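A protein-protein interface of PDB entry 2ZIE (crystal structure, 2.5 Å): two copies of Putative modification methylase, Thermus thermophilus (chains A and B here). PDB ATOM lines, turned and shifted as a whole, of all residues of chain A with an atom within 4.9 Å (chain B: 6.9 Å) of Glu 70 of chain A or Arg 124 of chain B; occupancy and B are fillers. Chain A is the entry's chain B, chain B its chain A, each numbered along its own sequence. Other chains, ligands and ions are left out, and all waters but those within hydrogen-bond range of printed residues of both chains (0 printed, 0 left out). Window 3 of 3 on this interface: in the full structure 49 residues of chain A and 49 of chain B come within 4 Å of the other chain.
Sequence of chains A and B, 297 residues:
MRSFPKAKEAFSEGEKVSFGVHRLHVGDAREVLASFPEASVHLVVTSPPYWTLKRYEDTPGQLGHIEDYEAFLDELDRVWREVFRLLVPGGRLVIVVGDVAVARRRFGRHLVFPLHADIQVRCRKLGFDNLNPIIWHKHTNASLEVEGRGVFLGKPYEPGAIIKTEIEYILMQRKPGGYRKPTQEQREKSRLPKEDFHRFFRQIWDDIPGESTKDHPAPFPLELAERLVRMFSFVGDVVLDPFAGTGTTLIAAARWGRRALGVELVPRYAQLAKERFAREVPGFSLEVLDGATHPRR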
ATOM      1  N   ILE A  66       1.632  14.664  20.342  1.00  0.00           N
ATOM      2  CA  ILE A  66       0.908  15.344  19.269  1.00  0.00           C
ATOM      3  C   ILE A  66       0.642  16.826  19.522  1.00  0.00           C
ATOM      4  O   ILE A  66       0.767  17.643  18.614  1.00  0.00           O
ATOM      5  CB  ILE A  66      -0.470  14.667  18.992  1.00  0.00           C
ATOM      6  CG1 ILE A  66      -0.285  13.183  18.656  1.00  0.00           C
ATOM      7  CG2 ILE A  66      -1.178  15.374  17.839  1.00  0.00           C
ATOM      8  CD1 ILE A  66       0.017  12.302  19.860  1.00  0.00           C
ATOM      9  N   GLU A  67       0.274  17.164  20.752  1.00  0.00           N
ATOM     10  CA  GLU A  67      -0.044  18.543  21.105  1.00  0.00           C
ATOM     11  C   GLU A  67       1.137  19.499  21.119  1.00  0.00           C
ATOM     12  O   GLU A  67       1.024  20.628  20.646  1.00  0.00           O
ATOM     13  CB  GLU A  67      -0.754  18.584  22.460  1.00  0.00           C
ATOM     14  CG  GLU A  67      -2.041  17.758  22.511  1.00  0.00           C
ATOM     15  CD  GLU A  67      -3.051  18.142  21.429  1.00  0.00           C
ATOM     16  OE1 GLU A  67      -4.144  17.532  21.406  1.00  0.00           O
ATOM     17  OE2 GLU A  67      -2.760  19.044  20.606  1.00  0.00           O
ATOM     18  N   ASP A  68       2.261  19.062  21.672  1.00  0.00           N
ATOM     19  CA  ASP A  68       3.447  19.908  21.714  1.00  0.00           C
ATOM     20  C   ASP A  68       3.908  20.137  20.279  1.00  0.00           C
ATOM     21  O   ASP A  68       4.318  21.236  19.901  1.00  0.00           O
ATOM     22  CB  ASP A  68       4.564  19.221  22.497  1.00  0.00           C
ATOM     23  CG  ASP A  68       4.111  18.742  23.860  1.00  0.00           C
ATOM     24  OD1 ASP A  68       3.231  17.850  23.922  1.00  0.00           O
ATOM     25  OD2 ASP A  68       4.637  19.262  24.867  1.00  0.00           O
ATOM     26  N   TYR A  69       3.830  19.073  19.489  1.00  0.00           N
ATOM     27  CA  TYR A  69       4.222  19.098  18.092  1.00  0.00           C
ATOM     28  C   TYR A  69       3.354  20.086  17.318  1.00  0.00           C
ATOM     29  O   TYR A  69       3.875  20.978  16.651  1.00  0.00           O
ATOM     30  CB  TYR A  69       4.086  17.688  17.510  1.00  0.00           C
ATOM     31  CG  TYR A  69       4.548  17.537  16.082  1.00  0.00           C
ATOM     32  CD1 TYR A  69       5.897  17.631  15.747  1.00  0.00           C
ATOM     33  CD2 TYR A  69       3.629  17.311  15.059  1.00  0.00           C
ATOM     34  CE1 TYR A  69       6.314  17.508  14.421  1.00  0.00           C
ATOM     35  CE2 TYR A  69       4.032  17.187  13.742  1.00  0.00           C
ATOM     36  CZ  TYR A  69       5.370  17.286  13.426  1.00  0.00           C
ATOM     37  OH  TYR A  69       5.761  17.163  12.118  1.00  0.00           O
ATOM     38  N   GLU A  70       2.033  19.930  17.412  1.00  0.00           N
ATOM     39  CA  GLU A  70       1.103  20.821  16.718  1.00  0.00           C
ATOM     40  C   GLU A  70       1.351  22.258  17.163  1.00  0.00           C
ATOM     41  O   GLU A  70       1.266  23.196  16.372  1.00  0.00           O
ATOM     42  CB  GLU A  70      -0.348  20.446  17.033  1.00  0.00           C
ATOM     43  CG  GLU A  70      -0.778  19.039  16.616  1.00  0.00           C
ATOM     44  CD  GLU A  70      -0.846  18.850  15.107  1.00  0.00           C
ATOM     45  OE1 GLU A  70      -1.543  19.643  14.433  1.00  0.00           O
ATOM     46  OE2 GLU A  70      -0.211  17.901  14.593  1.00  0.00           O
ATOM     47  N   ALA A  71       1.661  22.428  18.442  1.00  0.00           N
ATOM     48  CA  ALA A  71       1.922  23.749  18.988  1.00  0.00           C
ATOM     49  C   ALA A  71       3.164  24.350  18.344  1.00  0.00           C
ATOM     50  O   ALA A  71       3.172  25.521  17.964  1.00  0.00           O
ATOM     51  CB  ALA A  71       2.102  23.662  20.497  1.00  0.00           C
ATOM     52  N   PHE A  72       4.214  23.542  18.230  1.00  0.00           N
ATOM     53  CA  PHE A  72       5.464  23.988  17.625  1.00  0.00           C
ATOM     54  C   PHE A  72       5.217  24.426  16.188  1.00  0.00           C
ATOM     55  O   PHE A  72       5.698  25.467  15.753  1.00  0.00           O
ATOM     56  CB  PHE A  72       6.491  22.857  17.652  1.00  0.00           C
ATOM     57  CG  PHE A  72       7.814  23.219  17.037  1.00  0.00           C
ATOM     58  CD1 PHE A  72       8.537  24.313  17.500  1.00  0.00           C
ATOM     59  CD2 PHE A  72       8.347  22.454  16.003  1.00  0.00           C
ATOM     60  CE1 PHE A  72       9.773  24.639  16.945  1.00  0.00           C
ATOM     61  CE2 PHE A  72       9.580  22.769  15.442  1.00  0.00           C
ATOM     62  CZ  PHE A  72      10.297  23.862  15.911  1.00  0.00           C
ATOM     63  N   LEU A  73       4.455  23.629  15.455  1.00  0.00           N
ATOM     64  CA  LEU A  73       4.147  23.954  14.075  1.00  0.00           C
ATOM     65  C   LEU A  73       3.421  25.290  13.992  1.00  0.00           C
ATOM     66  O   LEU A  73       3.623  26.056  13.050  1.00  0.00           O
ATOM     67  CB  LEU A  73       3.282  22.854  13.451  1.00  0.00           C
ATOM     68  CG  LEU A  73       3.909  21.460  13.400  1.00  0.00           C
ATOM     69  CD1 LEU A  73       2.985  20.486  12.687  1.00  0.00           C
ATOM     70  CD2 LEU A  73       5.234  21.545  12.689  1.00  0.00           C
ATOM     71  N   ASP A  74       2.577  25.564  14.985  1.00  0.00           N
ATOM     72  CA  ASP A  74       1.814  26.802  15.022  1.00  0.00           C
ATOM     73  C   ASP A  74       2.746  27.995  15.167  1.00  0.00           C
ATOM     74  O   ASP A  74       2.564  29.017  14.500  1.00  0.00           O
ATOM     75  CB  ASP A  74       0.802  26.756  16.168  1.00  0.00           C
ATOM     76  CG  ASP A  74      -0.431  25.913  15.834  1.00  0.00           C
ATOM     77  OD1 ASP A  74      -1.177  25.558  16.775  1.00  0.00           O
ATOM     78  OD2 ASP A  74      -0.665  25.615  14.637  1.00  0.00           O
ATOM     79  N   PRO A 114       6.900  13.631  10.745  1.00  0.00           N
ATOM     80  CA  PRO A 114       7.197  14.127   9.399  1.00  0.00           C
ATOM     81  C   PRO A 114       7.263  15.647   9.309  1.00  0.00           C
ATOM     82  O   PRO A 114       6.542  16.268   8.531  1.00  0.00           O
ATOM     83  CB  PRO A 114       6.064  13.532   8.572  1.00  0.00           C
ATOM     84  CG  PRO A 114       4.914  13.608   9.517  1.00  0.00           C
ATOM     85  CD  PRO A 114       5.509  13.148  10.835  1.00  0.00           C
ATOM     86  N   ASP A 118       4.833  18.430   7.305  1.00  0.00           N
ATOM     87  CA  ASP A 118       3.949  19.350   8.003  1.00  0.00           C
ATOM     88  C   ASP A 118       4.257  20.783   7.637  1.00  0.00           C
ATOM     89  O   ASP A 118       3.345  21.584   7.429  1.00  0.00           O
ATOM     90  CB  ASP A 118       4.074  19.175   9.514  1.00  0.00           C
ATOM     91  CG  ASP A 118       3.176  18.090  10.041  1.00  0.00           C
ATOM     92  OD1 ASP A 118       1.950  18.190   9.812  1.00  0.00           O
ATOM     93  OD2 ASP A 118       3.688  17.146  10.679  1.00  0.00           O
ATOM     94  N   ARG A 122       1.667  23.267   5.682  1.00  0.00           N
ATOM     95  CA  ARG A 122       1.326  24.523   6.312  1.00  0.00           C
ATOM     96  C   ARG A 122       1.740  25.761   5.528  1.00  0.00           C
ATOM     97  O   ARG A 122       1.099  26.805   5.634  1.00  0.00           O
ATOM     98  CB  ARG A 122       1.895  24.553   7.727  1.00  0.00           C
ATOM     99  CG  ARG A 122       1.033  23.781   8.699  1.00  0.00           C
ATOM    100  CD  ARG A 122       1.818  23.358   9.902  1.00  0.00           C
ATOM    101  NE  ARG A 122       0.985  22.691  10.897  1.00  0.00           N
ATOM    102  CZ  ARG A 122       0.372  23.319  11.897  1.00  0.00           C
ATOM    103  NH1 ARG A 122       0.495  24.633  12.038  1.00  0.00           N
ATOM    104  NH2 ARG A 122      -0.356  22.632  12.763  1.00  0.00           N
ATOM    105  N   ILE B 119      -0.122  13.450   1.803  1.00  0.00           N
ATOM    106  CA  ILE B 119      -0.550  12.116   2.184  1.00  0.00           C
ATOM    107  C   ILE B 119       0.021  11.767   3.560  1.00  0.00           C
ATOM    108  O   ILE B 119      -0.677  11.194   4.396  1.00  0.00           O
ATOM    109  CB  ILE B 119      -0.103  11.079   1.158  1.00  0.00           C
ATOM    110  CG1 ILE B 119      -0.791  11.360  -0.175  1.00  0.00           C
ATOM    111  CG2 ILE B 119      -0.451   9.680   1.640  1.00  0.00           C
ATOM    112  CD1 ILE B 119      -0.361  10.443  -1.282  1.00  0.00           C
ATOM    113  N   GLN B 120       1.274  12.143   3.808  1.00  0.00           N
ATOM    114  CA  GLN B 120       1.910  11.847   5.088  1.00  0.00           C
ATOM    115  C   GLN B 120       1.141  12.448   6.249  1.00  0.00           C
ATOM    116  O   GLN B 120       0.818  11.753   7.217  1.00  0.00           O
ATOM    117  CB  GLN B 120       3.349  12.372   5.127  1.00  0.00           C
ATOM    118  CG  GLN B 120       4.377  11.399   4.591  1.00  0.00           C
ATOM    119  CD  GLN B 120       5.807  11.862   4.822  1.00  0.00           C
ATOM    120  OE1 GLN B 120       6.232  12.884   4.303  1.00  0.00           O
ATOM    121  NE2 GLN B 120       6.551  11.100   5.605  1.00  0.00           N
ATOM    122  N   VAL B 121       0.860  13.745   6.144  1.00  0.00           N
ATOM    123  CA  VAL B 121       0.144  14.466   7.177  1.00  0.00           C
ATOM    124  C   VAL B 121      -1.263  13.912   7.374  1.00  0.00           C
ATOM    125  O   VAL B 121      -1.682  13.637   8.497  1.00  0.00           O
ATOM    126  CB  VAL B 121       0.057  15.947   6.833  1.00  0.00           C
ATOM    127  CG1 VAL B 121      -0.783  16.666   7.874  1.00  0.00           C
ATOM    128  CG2 VAL B 121       1.453  16.547   6.773  1.00  0.00           C
ATOM    129  N   ARG B 122      -1.991  13.727   6.283  1.00  0.00           N
ATOM    130  CA  ARG B 122      -3.340  13.207   6.399  1.00  0.00           C
ATOM    131  C   ARG B 122      -3.367  11.801   7.002  1.00  0.00           C
ATOM    132  O   ARG B 122      -4.350  11.410   7.626  1.00  0.00           O
ATOM    133  CB  ARG B 122      -4.033  13.264   5.031  1.00  0.00           C
ATOM    134  CG  ARG B 122      -4.230  14.718   4.564  1.00  0.00           C
ATOM    135  CD  ARG B 122      -4.455  14.840   3.073  1.00  0.00           C
ATOM    136  NE  ARG B 122      -5.870  14.776   2.749  1.00  0.00           N
ATOM    137  CZ  ARG B 122      -6.711  15.801   2.843  1.00  0.00           C
ATOM    138  NH1 ARG B 122      -6.284  16.987   3.249  1.00  0.00           N
ATOM    139  NH2 ARG B 122      -7.982  15.628   2.533  1.00  0.00           N
ATOM    140  N   CYS B 123      -2.289  11.043   6.841  1.00  0.00           N
ATOM    141  CA  CYS B 123      -2.245   9.701   7.406  1.00  0.00           C
ATOM    142  C   CYS B 123      -2.081   9.751   8.918  1.00  0.00           C
ATOM    143  O   CYS B 123      -2.492   8.833   9.633  1.00  0.00           O
ATOM    144  CB  CYS B 123      -1.109   8.889   6.792  1.00  0.00           C
ATOM    145  SG  CYS B 123      -1.555   8.128   5.248  1.00  0.00           S
ATOM    146  N   ARG B 124      -1.468  10.820   9.407  1.00  0.00           N
ATOM    147  CA  ARG B 124      -1.292  10.954  10.838  1.00  0.00           C
ATOM    148  C   ARG B 124      -2.668  11.038  11.472  1.00  0.00           C
ATOM    149  O   ARG B 124      -2.954  10.352  12.446  1.00  0.00           O
ATOM    150  CB  ARG B 124      -0.483  12.205  11.168  1.00  0.00           C
ATOM    151  CG  ARG B 124      -0.400  12.505  12.646  1.00  0.00           C
ATOM    152  CD  ARG B 124       0.994  12.972  13.038  1.00  0.00           C
ATOM    153  NE  ARG B 124       1.476  14.063  12.197  1.00  0.00           N
ATOM    154  CZ  ARG B 124       0.883  15.245  12.092  1.00  0.00           C
ATOM    155  NH1 ARG B 124      -0.223  15.500  12.775  1.00  0.00           N
ATOM    156  NH2 ARG B 124       1.396  16.171  11.302  1.00  0.00           N
ATOM    157  N   LYS B 125      -3.532  11.858  10.888  1.00  0.00           N
ATOM    158  CA  LYS B 125      -4.878  12.038  11.409  1.00  0.00           C
ATOM    159  C   LYS B 125      -5.676  10.732  11.445  1.00  0.00           C
ATOM    160  O   LYS B 125      -6.572  10.580  12.268  1.00  0.00           O
ATOM    161  CB  LYS B 125      -5.617  13.085  10.571  1.00  0.00           C
ATOM    162  CG  LYS B 125      -6.702  13.848  11.322  1.00  0.00           C
ATOM    163  CD  LYS B 125      -7.261  14.994  10.464  1.00  0.00           C
ATOM    164  CE  LYS B 125      -8.081  15.998  11.288  1.00  0.00           C
ATOM    165  NZ  LYS B 125      -9.251  15.376  11.987  1.00  0.00           N
ATOM    166  N   LEU B 126      -5.353   9.793  10.558  1.00  0.00           N
ATOM    167  CA  LEU B 126      -6.057   8.514  10.512  1.00  0.00           C
ATOM    168  C   LEU B 126      -5.539   7.510  11.530  1.00  0.00           C
ATOM    169  O   LEU B 126      -6.087   6.419  11.666  1.00  0.00           O
ATOM    170  CB  LEU B 126      -5.960   7.904   9.116  1.00  0.00           C
ATOM    171  CG  LEU B 126      -6.911   8.431   8.042  1.00  0.00           C
ATOM    172  CD1 LEU B 126      -6.982   9.936   8.082  1.00  0.00           C
ATOM    173  CD2 LEU B 126      -6.430   7.960   6.685  1.00  0.00           C
ATOM    174  N   GLY B 127      -4.478   7.870  12.240  1.00  0.00           N
ATOM    175  CA  GLY B 127      -3.935   6.963  13.236  1.00  0.00           C
ATOM    176  C   GLY B 127      -2.644   6.241  12.876  1.00  0.00           C
ATOM    177  O   GLY B 127      -2.087   5.529  13.706  1.00  0.00           O
ATOM    178  N   PHE B 128      -2.163   6.418  11.649  1.00  0.00           N
ATOM    179  CA  PHE B 128      -0.928   5.773  11.213  1.00  0.00           C
ATOM    180  C   PHE B 128       0.287   6.381  11.879  1.00  0.00           C
ATOM    181  O   PHE B 128       0.304   7.573  12.177  1.00  0.00           O
ATOM    182  CB  PHE B 128      -0.739   5.937   9.702  1.00  0.00           C
ATOM    183  CG  PHE B 128      -1.587   5.033   8.870  1.00  0.00           C
ATOM    184  CD1 PHE B 128      -1.244   3.703   8.706  1.00  0.00           C
ATOM    185  CD2 PHE B 128      -2.710   5.522   8.219  1.00  0.00           C
ATOM    186  CE1 PHE B 128      -2.001   2.870   7.898  1.00  0.00           C
ATOM    187  CE2 PHE B 128      -3.478   4.694   7.409  1.00  0.00           C
ATOM    188  CZ  PHE B 128      -3.121   3.364   7.246  1.00  0.00           C
ATOM    189  N   ASP B 129       1.299   5.556  12.110  1.00  0.00           N
ATOM    190  CA  ASP B 129       2.558   6.030  12.658  1.00  0.00           C
ATOM    191  C   ASP B 129       3.431   6.261  11.432  1.00  0.00           C
ATOM    192  O   ASP B 129       3.536   5.399  10.563  1.00  0.00           O
ATOM    193  CB  ASP B 129       3.237   4.975  13.525  1.00  0.00           C
ATOM    194  CG  ASP B 129       2.768   5.001  14.961  1.00  0.00           C
ATOM    195  OD1 ASP B 129       2.199   6.027  15.402  1.00  0.00           O
ATOM    196  OD2 ASP B 129       2.993   3.991  15.658  1.00  0.00           O
ATOM    197  N   ASN B 130       4.056   7.420  11.350  1.00  0.00           N
ATOM    198  CA  ASN B 130       4.903   7.699  10.218  1.00  0.00           C
ATOM    199  C   ASN B 130       6.310   7.152  10.413  1.00  0.00           C
ATOM    200  O   ASN B 130       6.874   7.251  11.495  1.00  0.00           O
ATOM    201  CB  ASN B 130       4.980   9.200   9.978  1.00  0.00           C
ATOM    202  CG  ASN B 130       5.861   9.541   8.814  1.00  0.00           C
ATOM    203  OD1 ASN B 130       5.532   9.233   7.667  1.00  0.00           O
ATOM    204  ND2 ASN B 130       7.001  10.160   9.093  1.00  0.00           N
ATOM    205  N   GLN B 173       3.727   4.040   6.210  1.00  0.00           N
ATOM    206  CA  GLN B 173       2.834   4.309   7.325  1.00  0.00           C
ATOM    207  C   GLN B 173       2.534   3.024   8.053  1.00  0.00           C
ATOM    208  O   GLN B 173       2.022   2.064   7.480  1.00  0.00           O
ATOM    209  CB  GLN B 173       1.547   4.953   6.810  1.00  0.00           C
ATOM    210  CG  GLN B 173       1.798   6.197   5.982  1.00  0.00           C
ATOM    211  CD  GLN B 173       2.524   7.267   6.765  1.00  0.00           C
ATOM    212  OE1 GLN B 173       3.511   7.831   6.296  1.00  0.00           O
ATOM    213  NE2 GLN B 173       2.037   7.555   7.967  1.00  0.00           N
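Position printed for both chains: 122.
The side-chain amide nitrogen (NE2) of Gln 120 of chain B lies within hydrogen-bond range of the side-chain amide oxygen (OD1) of Asn 130 of chain B (3.0 Å). OD1 of Asn 130 of chain B sits close to OE1 of Gln 173 of chain B, at 2.8 Å. The side-chain hydroxyl (OH) of Tyr 69 of chain A sits at hydrogen-bond distance from the side-chain carboxylate (OD2) of Asp 118 of chain A (2.5 Å). The guanidinium group of Arg 122 of chain A lies within salt-bridge range of the side-chain carboxylate of Glu 70 of chain A (3.6 Å).
Among the printed residues, merely in contact across the chains: Tyr 69 of chain A with Arg 124 of chain B (3.7 Å), Pro 114 of chain A with Gln 120 of chain B (3.9 Å), Pro 114 of chain A with Asn 130 of chain B (3.5 Å) and Asp 118 of chain A with Val 121 of chain B (3.5 Å).
Hydrophobic or aromatic side chains of chain A that line the printed part of chain B: Tyr 69 and Pro 114. Of the 13 printed residues of chain B, 4 touch a printed residue of chain A. Along chain B the printed residues that touch a printed residue of chain A span positions 120 to 130. Among the printed residues, Asp or Glu carboxylates within 4 Å of a Lys or Arg side-chain nitrogen of the other chain: Glu 70 of chain A with Arg 124 of chain B (3.0 Å) and Asp 118 of chain A with Arg 124 of chain B (2.6 Å).
NH1 of Arg 124 of chain B lies within salt-bridge range of OE2 of Glu 70 of chain A. The side-chain carboxylate of Asp 118 of chain A lies within salt-bridge range of the guanidinium group of Arg 124 of chain B (2.6 Å).
Of chain A, only Tyr 69, Glu 70 and Asp 118 come within 4 Å of Arg 124 of chain B. Printed residues of chain A within 4 Å of Asn 130 of chain B: Pro 114 (3.5 Å). Printed residues of chain B within 4 Å of Tyr 69 of chain A: Arg 124 (3.7 Å). Printed residues of chain B within 4 Å of Pro 114 of chain A: Gln 120 and Asn 130. Of the printed residues of chain A, Val 121 of chain B touches Asp 118 (3.5 Å). The nearest printed residue of chain B that does not touch Glu 70 of chain A is Val 121 of chain B (6.9 Å). The nearest printed residue of chain A that does not touch Asn 130 of chain B is Tyr 69 of chain A (7.7 Å).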
